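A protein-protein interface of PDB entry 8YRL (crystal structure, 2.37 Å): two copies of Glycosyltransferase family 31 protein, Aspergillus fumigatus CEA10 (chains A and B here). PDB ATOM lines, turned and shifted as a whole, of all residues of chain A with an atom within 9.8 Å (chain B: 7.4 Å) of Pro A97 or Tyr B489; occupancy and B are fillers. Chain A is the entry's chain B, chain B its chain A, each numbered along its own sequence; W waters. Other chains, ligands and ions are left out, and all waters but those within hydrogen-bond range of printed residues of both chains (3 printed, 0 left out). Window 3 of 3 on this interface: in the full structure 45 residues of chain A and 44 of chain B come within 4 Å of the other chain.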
ATOM      1  N   TRP A  50       1.452  32.377 -11.717  1.00  0.00           N
ATOM      2  CA  TRP A  50       2.390  31.609 -12.531  1.00  0.00           C
ATOM      3  C   TRP A  50       3.814  31.732 -12.002  1.00  0.00           C
ATOM      4  O   TRP A  50       4.580  30.761 -12.035  1.00  0.00           O
ATOM      5  CB  TRP A  50       2.312  32.084 -13.983  1.00  0.00           C
ATOM      6  CG  TRP A  50       3.124  31.275 -14.952  1.00  0.00           C
ATOM      7  CD1 TRP A  50       2.711  30.186 -15.660  1.00  0.00           C
ATOM      8  CD2 TRP A  50       4.487  31.506 -15.328  1.00  0.00           C
ATOM      9  NE1 TRP A  50       3.735  29.719 -16.451  1.00  0.00           N
ATOM     10  CE2 TRP A  50       4.836  30.513 -16.266  1.00  0.00           C
ATOM     11  CE3 TRP A  50       5.449  32.452 -14.962  1.00  0.00           C
ATOM     12  CZ2 TRP A  50       6.103  30.440 -16.841  1.00  0.00           C
ATOM     13  CZ3 TRP A  50       6.704  32.382 -15.536  1.00  0.00           C
ATOM     14  CH2 TRP A  50       7.021  31.381 -16.462  1.00  0.00           C
ATOM     15  N   LEU A  51       4.183  32.917 -11.505  1.00  0.00           N
ATOM     16  CA  LEU A  51       5.574  33.150 -11.111  1.00  0.00           C
ATOM     17  C   LEU A  51       5.977  32.388  -9.854  1.00  0.00           C
ATOM     18  O   LEU A  51       7.017  31.706  -9.882  1.00  0.00           O
ATOM     19  CB  LEU A  51       5.821  34.654 -10.964  1.00  0.00           C
ATOM     20  CG  LEU A  51       5.937  35.451 -12.266  1.00  0.00           C
ATOM     21  CD1 LEU A  51       5.780  36.941 -12.001  1.00  0.00           C
ATOM     22  CD2 LEU A  51       7.258  35.163 -12.961  1.00  0.00           C
ATOM     23  N   PRO A  52       5.248  32.452  -8.736  1.00  0.00           N
ATOM     24  CA  PRO A  52       5.762  31.854  -7.500  1.00  0.00           C
ATOM     25  C   PRO A  52       5.682  30.336  -7.513  1.00  0.00           C
ATOM     26  O   PRO A  52       4.936  29.723  -8.279  1.00  0.00           O
ATOM     27  CB  PRO A  52       4.849  32.437  -6.419  1.00  0.00           C
ATOM     28  CG  PRO A  52       3.567  32.669  -7.117  1.00  0.00           C
ATOM     29  CD  PRO A  52       3.924  33.073  -8.521  1.00  0.00           C
ATOM     30  N   ARG A  53       6.486  29.731  -6.638  1.00  0.00           N
ATOM     31  CA  ARG A  53       6.308  28.327  -6.305  1.00  0.00           C
ATOM     32  C   ARG A  53       5.072  28.169  -5.429  1.00  0.00           C
ATOM     33  O   ARG A  53       4.674  29.089  -4.709  1.00  0.00           O
ATOM     34  CB  ARG A  53       7.537  27.780  -5.579  1.00  0.00           C
ATOM     35  CG  ARG A  53       8.864  28.097  -6.250  1.00  0.00           C
ATOM     36  CD  ARG A  53      10.035  27.607  -5.407  1.00  0.00           C
ATOM     37  NE  ARG A  53      10.092  26.151  -5.333  1.00  0.00           N
ATOM     38  CZ  ARG A  53       9.728  25.438  -4.276  1.00  0.00           C
ATOM     39  NH1 ARG A  53       9.262  26.015  -3.181  1.00  0.00           N
ATOM     40  NH2 ARG A  53       9.830  24.114  -4.320  1.00  0.00           N
ATOM     41  N   THR A  87       0.654  18.560  -4.330  1.00  0.00           N
ATOM     42  CA  THR A  87       1.847  18.426  -5.155  1.00  0.00           C
ATOM     43  C   THR A  87       2.619  19.738  -5.136  1.00  0.00           C
ATOM     44  O   THR A  87       2.047  20.804  -5.386  1.00  0.00           O
ATOM     45  CB  THR A  87       1.484  18.048  -6.594  1.00  0.00           C
ATOM     46  OG1 THR A  87       0.725  16.833  -6.594  1.00  0.00           O
ATOM     47  CG2 THR A  87       2.740  17.854  -7.429  1.00  0.00           C
ATOM     48  N   VAL A  88       3.911  19.657  -4.835  1.00  0.00           N
ATOM     49  CA  VAL A  88       4.775  20.834  -4.825  1.00  0.00           C
ATOM     50  C   VAL A  88       5.086  21.221  -6.263  1.00  0.00           C
ATOM     51  O   VAL A  88       5.660  20.431  -7.020  1.00  0.00           O
ATOM     52  CB  VAL A  88       6.062  20.570  -4.032  1.00  0.00           C
ATOM     53  CG1 VAL A  88       7.005  21.760  -4.135  1.00  0.00           C
ATOM     54  CG2 VAL A  88       5.738  20.269  -2.578  1.00  0.00           C
ATOM     55  N   LEU A  89       4.707  22.437  -6.646  1.00  0.00           N
ATOM     56  CA  LEU A  89       4.938  22.943  -7.990  1.00  0.00           C
ATOM     57  C   LEU A  89       5.923  24.102  -7.954  1.00  0.00           C
ATOM     58  O   LEU A  89       5.938  24.891  -7.003  1.00  0.00           O
ATOM     59  CB  LEU A  89       3.632  23.402  -8.646  1.00  0.00           C
ATOM     60  CG  LEU A  89       2.557  22.343  -8.907  1.00  0.00           C
ATOM     61  CD1 LEU A  89       1.465  22.916  -9.795  1.00  0.00           C
ATOM     62  CD2 LEU A  89       3.157  21.094  -9.533  1.00  0.00           C
ATOM     63  N   GLU A  90       6.746  24.195  -8.998  1.00  0.00           N
ATOM     64  CA  GLU A  90       7.672  25.309  -9.147  1.00  0.00           C
ATOM     65  C   GLU A  90       6.992  26.465  -9.866  1.00  0.00           C
ATOM     66  O   GLU A  90       5.794  26.704  -9.685  1.00  0.00           O
ATOM     67  CB  GLU A  90       8.925  24.871  -9.911  1.00  0.00           C
ATOM     68  CG  GLU A  90       9.726  23.775  -9.229  1.00  0.00           C
ATOM     69  CD  GLU A  90      10.472  24.271  -8.006  1.00  0.00           C
ATOM     70  OE1 GLU A  90      10.694  25.495  -7.896  1.00  0.00           O
ATOM     71  OE2 GLU A  90      10.841  23.436  -7.154  1.00  0.00           O
ATOM     72  N   ARG A  91       7.752  27.183 -10.686  1.00  0.00           N
ATOM     73  CA  ARG A  91       7.180  28.246 -11.496  1.00  0.00           C
ATOM     74  C   ARG A  91       6.326  27.655 -12.610  1.00  0.00           C
ATOM     75  O   ARG A  91       6.711  26.676 -13.256  1.00  0.00           O
ATOM     76  CB  ARG A  91       8.294  29.118 -12.076  1.00  0.00           C
ATOM     77  CG  ARG A  91       7.818  30.289 -12.909  1.00  0.00           C
ATOM     78  CD  ARG A  91       8.959  31.256 -13.178  1.00  0.00           C
ATOM     79  NE  ARG A  91       9.316  32.026 -11.992  1.00  0.00           N
ATOM     80  CZ  ARG A  91      10.057  33.125 -12.011  1.00  0.00           C
ATOM     81  NH1 ARG A  91      10.548  33.608 -13.140  1.00  0.00           N
ATOM     82  NH2 ARG A  91      10.314  33.754 -10.866  1.00  0.00           N
ATOM     83  N   GLY A  92       5.157  28.248 -12.828  1.00  0.00           N
ATOM     84  CA  GLY A  92       4.239  27.723 -13.828  1.00  0.00           C
ATOM     85  C   GLY A  92       3.447  26.564 -13.266  1.00  0.00           C
ATOM     86  O   GLY A  92       2.824  26.680 -12.211  1.00  0.00           O
ATOM     87  N   MET A  93       3.459  25.438 -13.979  1.00  0.00           N
ATOM     88  CA  MET A  93       2.868  24.197 -13.490  1.00  0.00           C
ATOM     89  C   MET A  93       3.890  23.066 -13.456  1.00  0.00           C
ATOM     90  O   MET A  93       3.514  21.890 -13.513  1.00  0.00           O
ATOM     91  CB  MET A  93       1.659  23.801 -14.338  1.00  0.00           C
ATOM     92  CG  MET A  93       0.475  24.750 -14.217  1.00  0.00           C
ATOM     93  SD  MET A  93      -0.104  24.951 -12.519  1.00  0.00           S
ATOM     94  CE  MET A  93      -1.117  23.487 -12.334  1.00  0.00           C
ATOM     95  N   VAL A  94       5.176  23.403 -13.358  1.00  0.00           N
ATOM     96  CA  VAL A  94       6.225  22.395 -13.382  1.00  0.00           C
ATOM     97  C   VAL A  94       6.220  21.625 -12.070  1.00  0.00           C
ATOM     98  O   VAL A  94       6.280  22.214 -10.982  1.00  0.00           O
ATOM     99  CB  VAL A  94       7.590  23.052 -13.638  1.00  0.00           C
ATOM    100  CG1 VAL A  94       8.708  22.033 -13.491  1.00  0.00           C
ATOM    101  CG2 VAL A  94       7.616  23.694 -15.018  1.00  0.00           C
ATOM    102  N   VAL A  95       6.138  20.299 -12.165  1.00  0.00           N
ATOM    103  CA  VAL A  95       6.208  19.449 -10.983  1.00  0.00           C
ATOM    104  C   VAL A  95       7.624  19.502 -10.425  1.00  0.00           C
ATOM    105  O   VAL A  95       8.598  19.221 -11.133  1.00  0.00           O
ATOM    106  CB  VAL A  95       5.792  18.011 -11.315  1.00  0.00           C
ATOM    107  CG1 VAL A  95       5.913  17.127 -10.086  1.00  0.00           C
ATOM    108  CG2 VAL A  95       4.370  17.984 -11.861  1.00  0.00           C
ATOM    109  N   SER A  96       7.744  19.866  -9.151  1.00  0.00           N
ATOM    110  CA  SER A  96       9.049  20.046  -8.543  1.00  0.00           C
ATOM    111  C   SER A  96       9.719  18.698  -8.284  1.00  0.00           C
ATOM    112  O   SER A  96       9.042  17.693  -8.054  1.00  0.00           O
ATOM    113  CB  SER A  96       8.919  20.816  -7.232  1.00  0.00           C
ATOM    114  OG  SER A  96      10.043  20.598  -6.396  1.00  0.00           O
ATOM    115  N   PRO A  97      11.056  18.648  -8.325  1.00  0.00           N
ATOM    116  CA  PRO A  97      11.753  17.426  -7.894  1.00  0.00           C
ATOM    117  C   PRO A  97      11.581  17.133  -6.417  1.00  0.00           C
ATOM    118  O   PRO A  97      11.845  16.000  -5.989  1.00  0.00           O
ATOM    119  CB  PRO A  97      13.220  17.713  -8.243  1.00  0.00           C
ATOM    120  CG  PRO A  97      13.315  19.207  -8.289  1.00  0.00           C
ATOM    121  CD  PRO A  97      11.989  19.676  -8.814  1.00  0.00           C
ATOM    122  N   ASP A  98      11.138  18.109  -5.628  1.00  0.00           N
ATOM    123  CA  ASP A  98      10.777  17.889  -4.229  1.00  0.00           C
ATOM    124  C   ASP A  98       9.446  17.165  -4.077  1.00  0.00           C
ATOM    125  O   ASP A  98       8.643  17.513  -3.208  1.00  0.00           O
ATOM    126  CB  ASP A  98      10.744  19.234  -3.510  1.00  0.00           C
ATOM    127  CG  ASP A  98      10.926  19.100  -2.016  1.00  0.00           C
ATOM    128  OD1 ASP A  98      11.697  18.217  -1.589  1.00  0.00           O
ATOM    129  OD2 ASP A  98      10.299  19.875  -1.263  1.00  0.00           O
ATOM    130  N   ASN A  99       9.192  16.153  -4.906  1.00  0.00           N
ATOM    131  CA  ASN A  99       7.912  15.464  -4.947  1.00  0.00           C
ATOM    132  C   ASN A  99       8.124  13.957  -4.984  1.00  0.00           C
ATOM    133  O   ASN A  99       9.103  13.459  -5.547  1.00  0.00           O
ATOM    134  CB  ASN A  99       7.087  15.889  -6.172  1.00  0.00           C
ATOM    135  CG  ASN A  99       6.118  17.018  -5.868  1.00  0.00           C
ATOM    136  OD1 ASN A  99       5.457  17.024  -4.829  1.00  0.00           O
ATOM    137  ND2 ASN A  99       6.041  17.987  -6.772  1.00  0.00           N
ATOM    138  N   LYS A 100       7.175  13.239  -4.385  1.00  0.00           N
ATOM    139  CA  LYS A 100       7.180  11.782  -4.442  1.00  0.00           C
ATOM    140  C   LYS A 100       7.047  11.290  -5.877  1.00  0.00           C
ATOM    141  O   LYS A 100       7.775  10.390  -6.310  1.00  0.00           O
ATOM    142  CB  LYS A 100       6.051  11.222  -3.570  1.00  0.00           C
ATOM    143  CG  LYS A 100       5.889  11.888  -2.197  1.00  0.00           C
ATOM    144  CD  LYS A 100       5.002  13.150  -2.191  1.00  0.00           C
ATOM    145  CE  LYS A 100       3.549  12.875  -2.562  1.00  0.00           C
ATOM    146  NZ  LYS A 100       2.752  14.130  -2.610  1.00  0.00           N
ATOM    147  N   ASP A 101       6.118  11.873  -6.632  1.00  0.00           N
ATOM    148  CA  ASP A 101       5.845  11.483  -8.003  1.00  0.00           C
ATOM    149  C   ASP A 101       6.178  12.621  -8.961  1.00  0.00           C
ATOM    150  O   ASP A 101       6.023  13.796  -8.613  1.00  0.00           O
ATOM    151  CB  ASP A 101       4.373  11.083  -8.178  1.00  0.00           C
ATOM    152  CG  ASP A 101       3.965   9.947  -7.261  1.00  0.00           C
ATOM    153  OD1 ASP A 101       4.613   8.881  -7.308  1.00  0.00           O
ATOM    154  OD2 ASP A 101       2.998  10.124  -6.490  1.00  0.00           O
ATOM    155  N   PRO A 102       6.641  12.306 -10.172  1.00  0.00           N
ATOM    156  CA  PRO A 102       6.983  13.355 -11.141  1.00  0.00           C
ATOM    157  C   PRO A 102       5.792  13.954 -11.870  1.00  0.00           C
ATOM    158  O   PRO A 102       5.990  14.825 -12.725  1.00  0.00           O
ATOM    159  CB  PRO A 102       7.901  12.609 -12.120  1.00  0.00           C
ATOM    160  CG  PRO A 102       7.342  11.228 -12.120  1.00  0.00           C
ATOM    161  CD  PRO A 102       6.998  10.966 -10.674  1.00  0.00           C
ATOM    162  N   SER A 103       4.569  13.524 -11.568  1.00  0.00           N
ATOM    163  CA  SER A 103       3.389  13.975 -12.286  1.00  0.00           C
ATOM    164  C   SER A 103       2.308  14.405 -11.305  1.00  0.00           C
ATOM    165  O   SER A 103       2.314  14.026 -10.131  1.00  0.00           O
ATOM    166  CB  SER A 103       2.842  12.879 -13.212  1.00  0.00           C
ATOM    167  OG  SER A 103       2.187  13.440 -14.336  1.00  0.00           O
ATOM    168  N   ASN B 150      14.297  32.581  -9.643  1.00  0.00           N
ATOM    169  CA  ASN B 150      14.875  31.588 -10.551  1.00  0.00           C
ATOM    170  C   ASN B 150      16.124  32.112 -11.256  1.00  0.00           C
ATOM    171  O   ASN B 150      16.395  31.762 -12.406  1.00  0.00           O
ATOM    172  CB  ASN B 150      13.844  31.096 -11.572  1.00  0.00           C
ATOM    173  CG  ASN B 150      12.868  30.104 -10.975  1.00  0.00           C
ATOM    174  OD1 ASN B 150      12.688  30.050  -9.758  1.00  0.00           O
ATOM    175  ND2 ASN B 150      12.234  29.309 -11.828  1.00  0.00           N
ATOM    176  N   THR B 151      16.885  32.958 -10.571  1.00  0.00           N
ATOM    177  CA  THR B 151      18.213  33.365 -11.001  1.00  0.00           C
ATOM    178  C   THR B 151      19.211  33.024  -9.902  1.00  0.00           C
ATOM    179  O   THR B 151      18.837  32.640  -8.792  1.00  0.00           O
ATOM    180  CB  THR B 151      18.271  34.864 -11.329  1.00  0.00           C
ATOM    181  OG1 THR B 151      18.245  35.622 -10.112  1.00  0.00           O
ATOM    182  CG2 THR B 151      17.094  35.270 -12.203  1.00  0.00           C
ATOM    183  N   GLY B 485      12.174  32.142 -17.028  1.00  0.00           N
ATOM    184  CA  GLY B 485      12.658  31.378 -15.895  1.00  0.00           C
ATOM    185  C   GLY B 485      11.866  30.137 -15.561  1.00  0.00           C
ATOM    186  O   GLY B 485      11.897  29.688 -14.412  1.00  0.00           O
ATOM    187  N   VAL B 486      11.158  29.558 -16.531  1.00  0.00           N
ATOM    188  CA  VAL B 486      10.365  28.367 -16.242  1.00  0.00           C
ATOM    189  C   VAL B 486      11.249  27.126 -16.147  1.00  0.00           C
ATOM    190  O   VAL B 486      10.889  26.154 -15.471  1.00  0.00           O
ATOM    191  CB  VAL B 486       9.253  28.197 -17.293  1.00  0.00           C
ATOM    192  CG1 VAL B 486       9.824  27.698 -18.614  1.00  0.00           C
ATOM    193  CG2 VAL B 486       8.167  27.258 -16.778  1.00  0.00           C
ATOM    194  N   HIS B 487      12.412  27.134 -16.796  1.00  0.00           N
ATOM    195  CA  HIS B 487      13.337  26.011 -16.757  1.00  0.00           C
ATOM    196  C   HIS B 487      14.471  26.214 -15.761  1.00  0.00           C
ATOM    197  O   HIS B 487      15.349  25.350 -15.658  1.00  0.00           O
ATOM    198  CB  HIS B 487      13.923  25.755 -18.151  1.00  0.00           C
ATOM    199  CG  HIS B 487      12.894  25.676 -19.237  1.00  0.00           C
ATOM    200  ND1 HIS B 487      12.841  26.576 -20.279  1.00  0.00           N
ATOM    201  CD2 HIS B 487      11.882  24.801 -19.445  1.00  0.00           C
ATOM    202  CE1 HIS B 487      11.839  26.260 -21.081  1.00  0.00           C
ATOM    203  NE2 HIS B 487      11.241  25.186 -20.596  1.00  0.00           N
ATOM    204  N   ASP B 488      14.474  27.322 -15.024  1.00  0.00           N
ATOM    205  CA  ASP B 488      15.557  27.674 -14.113  1.00  0.00           C
ATOM    206  C   ASP B 488      15.138  27.533 -12.652  1.00  0.00           C
ATOM    207  O   ASP B 488      15.535  28.328 -11.799  1.00  0.00           O
ATOM    208  CB  ASP B 488      16.047  29.094 -14.385  1.00  0.00           C
ATOM    209  CG  ASP B 488      16.534  29.281 -15.807  1.00  0.00           C
ATOM    210  OD1 ASP B 488      17.185  28.359 -16.341  1.00  0.00           O
ATOM    211  OD2 ASP B 488      16.262  30.349 -16.394  1.00  0.00           O
ATOM    212  N   TYR B 489      14.337  26.511 -12.342  1.00  0.00           N
ATOM    213  CA  TYR B 489      13.844  26.355 -10.978  1.00  0.00           C
ATOM    214  C   TYR B 489      14.872  25.705 -10.060  1.00  0.00           C
ATOM    215  O   TYR B 489      14.887  25.993  -8.857  1.00  0.00           O
ATOM    216  CB  TYR B 489      12.541  25.551 -10.968  1.00  0.00           C
ATOM    217  CG  TYR B 489      12.622  24.181 -11.611  1.00  0.00           C
ATOM    218  CD1 TYR B 489      13.059  23.078 -10.889  1.00  0.00           C
ATOM    219  CD2 TYR B 489      12.244  23.991 -12.934  1.00  0.00           C
ATOM    220  CE1 TYR B 489      13.127  21.825 -11.470  1.00  0.00           C
ATOM    221  CE2 TYR B 489      12.308  22.742 -13.522  1.00  0.00           C
ATOM    222  CZ  TYR B 489      12.751  21.664 -12.787  1.00  0.00           C
ATOM    223  OH  TYR B 489      12.814  20.420 -13.369  1.00  0.00           O
ATOM    224  N   ALA B 490      15.730  24.838 -10.593  1.00  0.00           N
ATOM    225  CA  ALA B 490      16.778  24.190  -9.813  1.00  0.00           C
ATOM    226  C   ALA B 490      18.131  24.872  -9.978  1.00  0.00           C
ATOM    227  O   ALA B 490      19.169  24.245  -9.745  1.00  0.00           O
ATOM    228  CB  ALA B 490      16.881  22.712 -10.193  1.00  0.00           C
ATOM    229  N   VAL B 491      18.137  26.149 -10.362  1.00  0.00           N
ATOM    230  CA  VAL B 491      19.389  26.824 -10.690  1.00  0.00           C
ATOM    231  C   VAL B 491      20.128  27.324  -9.453  1.00  0.00           C
ATOM    232  O   VAL B 491      21.326  27.624  -9.535  1.00  0.00           O
ATOM    233  CB  VAL B 491      19.101  27.956 -11.691  1.00  0.00           C
ATOM    234  CG1 VAL B 491      19.211  29.330 -11.034  1.00  0.00           C
ATOM    235  CG2 VAL B 491      20.034  27.838 -12.879  1.00  0.00           C
ATOM    236  N   ARG B 492      19.457  27.402  -8.305  1.00  0.00           N
ATOM    237  CA  ARG B 492      20.081  27.786  -7.046  1.00  0.00           C
ATOM    238  C   ARG B 492      20.419  26.584  -6.174  1.00  0.00           C
ATOM    239  O   ARG B 492      20.825  26.763  -5.020  1.00  0.00           O
ATOM    240  CB  ARG B 492      19.168  28.744  -6.280  1.00  0.00           C
ATOM    241  CG  ARG B 492      18.635  29.883  -7.126  1.00  0.00           C
ATOM    242  CD  ARG B 492      17.970  30.966  -6.286  1.00  0.00           C
ATOM    243  NE  ARG B 492      18.821  31.516  -5.237  1.00  0.00           N
ATOM    244  CZ  ARG B 492      19.470  32.670  -5.326  1.00  0.00           C
ATOM    245  NH1 ARG B 492      19.461  33.386  -6.439  1.00  0.00           N
ATOM    246  NH2 ARG B 492      20.140  33.120  -4.270  1.00  0.00           N
ATOM    247  N   LYS B 493      20.271  25.371  -6.698  1.00  0.00           N
ATOM    248  CA  LYS B 493      20.431  24.167  -5.900  1.00  0.00           C
ATOM    249  C   LYS B 493      21.903  23.783  -5.773  1.00  0.00           C
ATOM    250  O   LYS B 493      22.744  24.137  -6.606  1.00  0.00           O
ATOM    251  CB  LYS B 493      19.628  23.014  -6.509  1.00  0.00           C
ATOM    252  CG  LYS B 493      20.455  21.942  -7.202  1.00  0.00           C
ATOM    253  CD  LYS B 493      19.582  20.766  -7.606  1.00  0.00           C
ATOM    254  CE  LYS B 493      19.270  19.878  -6.412  1.00  0.00           C
ATOM    255  NZ  LYS B 493      18.897  18.498  -6.825  1.00  0.00           N
HETATM  256  O   HOH W   1      10.570  27.878  -9.484  1.00  0.00           O
HETATM  257  O   HOH W   2       9.595  26.297 -13.062  1.00  0.00           O
HETATM  258  O   HOH W   3      11.470  31.936  -8.377  1.00  0.00           O
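O of Gly B485 is in hydrogen-bond range of ND2 of Asn B150 (2.6 Å). The side-chain amide nitrogen of Asn B150 sits close to the backbone carbonyl oxygen of Asp B488, 3.4 Å away. O of Trp A50 is in hydrogen-bond range of N of Gly A92 (2.7 Å). O of Leu A51 is in hydrogen-bond range of NE of Arg A91 (3.1 Å). The side-chain carboxylate (OE1) of Glu A90 lies within salt-bridge range of the guanidinium group (NE) of Arg A53 (2.7 Å). OE2 of Glu A90 sits at hydrogen-bond distance from OG of Ser A96, at 3.0 Å.
Among the printed residues, merely in contact across the chains: Trp A50 with Val B486 (3.8 Å), Glu A90 with Tyr B489 (3.6 Å), Arg A91 with Asn B150 (3.95 Å), Arg A91 with Gly B485 (3.6 Å), Arg A91 with Val B486 (3.9 Å), Val A94 with Tyr B489 (3.7 Å) and Pro A97 with Tyr B489 (3.6 Å).
Pro A97 touches just one residue of chain B: Tyr B489 (3.6 Å). Tyr B489 touches just these residues of chain A: Glu A90 (3.6 Å), Val A94 (3.7 Å) and Pro A97 (3.6 Å). Printed residues of chain B within 4 Å of Val A94: Tyr B489 (3.7 Å). Printed residues of chain A within 4 Å of Asn B150: Arg A91. Pro A102 touches none of the printed residues of chain B. The nearest residue of chain B that does not touch Pro A97 is Ala B490 (5.4 Å). The nearest printed residue of chain B that does not touch Trp A50 is Gly B485 (5.1 Å).
Printed residues of chain A that touch a printed residue of chain B: Trp A50, Glu A90, Arg A91, Val A94 and Pro A97. Hydrophobic or aromatic side chains of chain A within 4 Å of the printed part of chain B: Trp A50, Val A94 and Pro A97. Of the 11 printed residues of chain B, 4 touch a printed residue of chain A. Among the printed residues, no Asp or Glu carboxylate lies within 4 Å of a Lys or Arg side-chain nitrogen of the other chain.
No position is printed for both chains.
Water W3 bridges OD1 of Asn B150 (2.6 Å) and NH2 of Arg A91 (3.3 Å). Water W2 bridges the backbone carbonyl oxygen (O) of Val B486 and the backbone carbonyl oxygen (O) of Arg A91. Water W1 lies within hydrogen-bond range of the side-chain carboxylate (OE1) of Glu A90 (2.9 Å), the side-chain amide oxygen (OD1) of Asn B150 (3.0 Å) and the backbone NH (N) of Arg A91 (3.1 Å).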
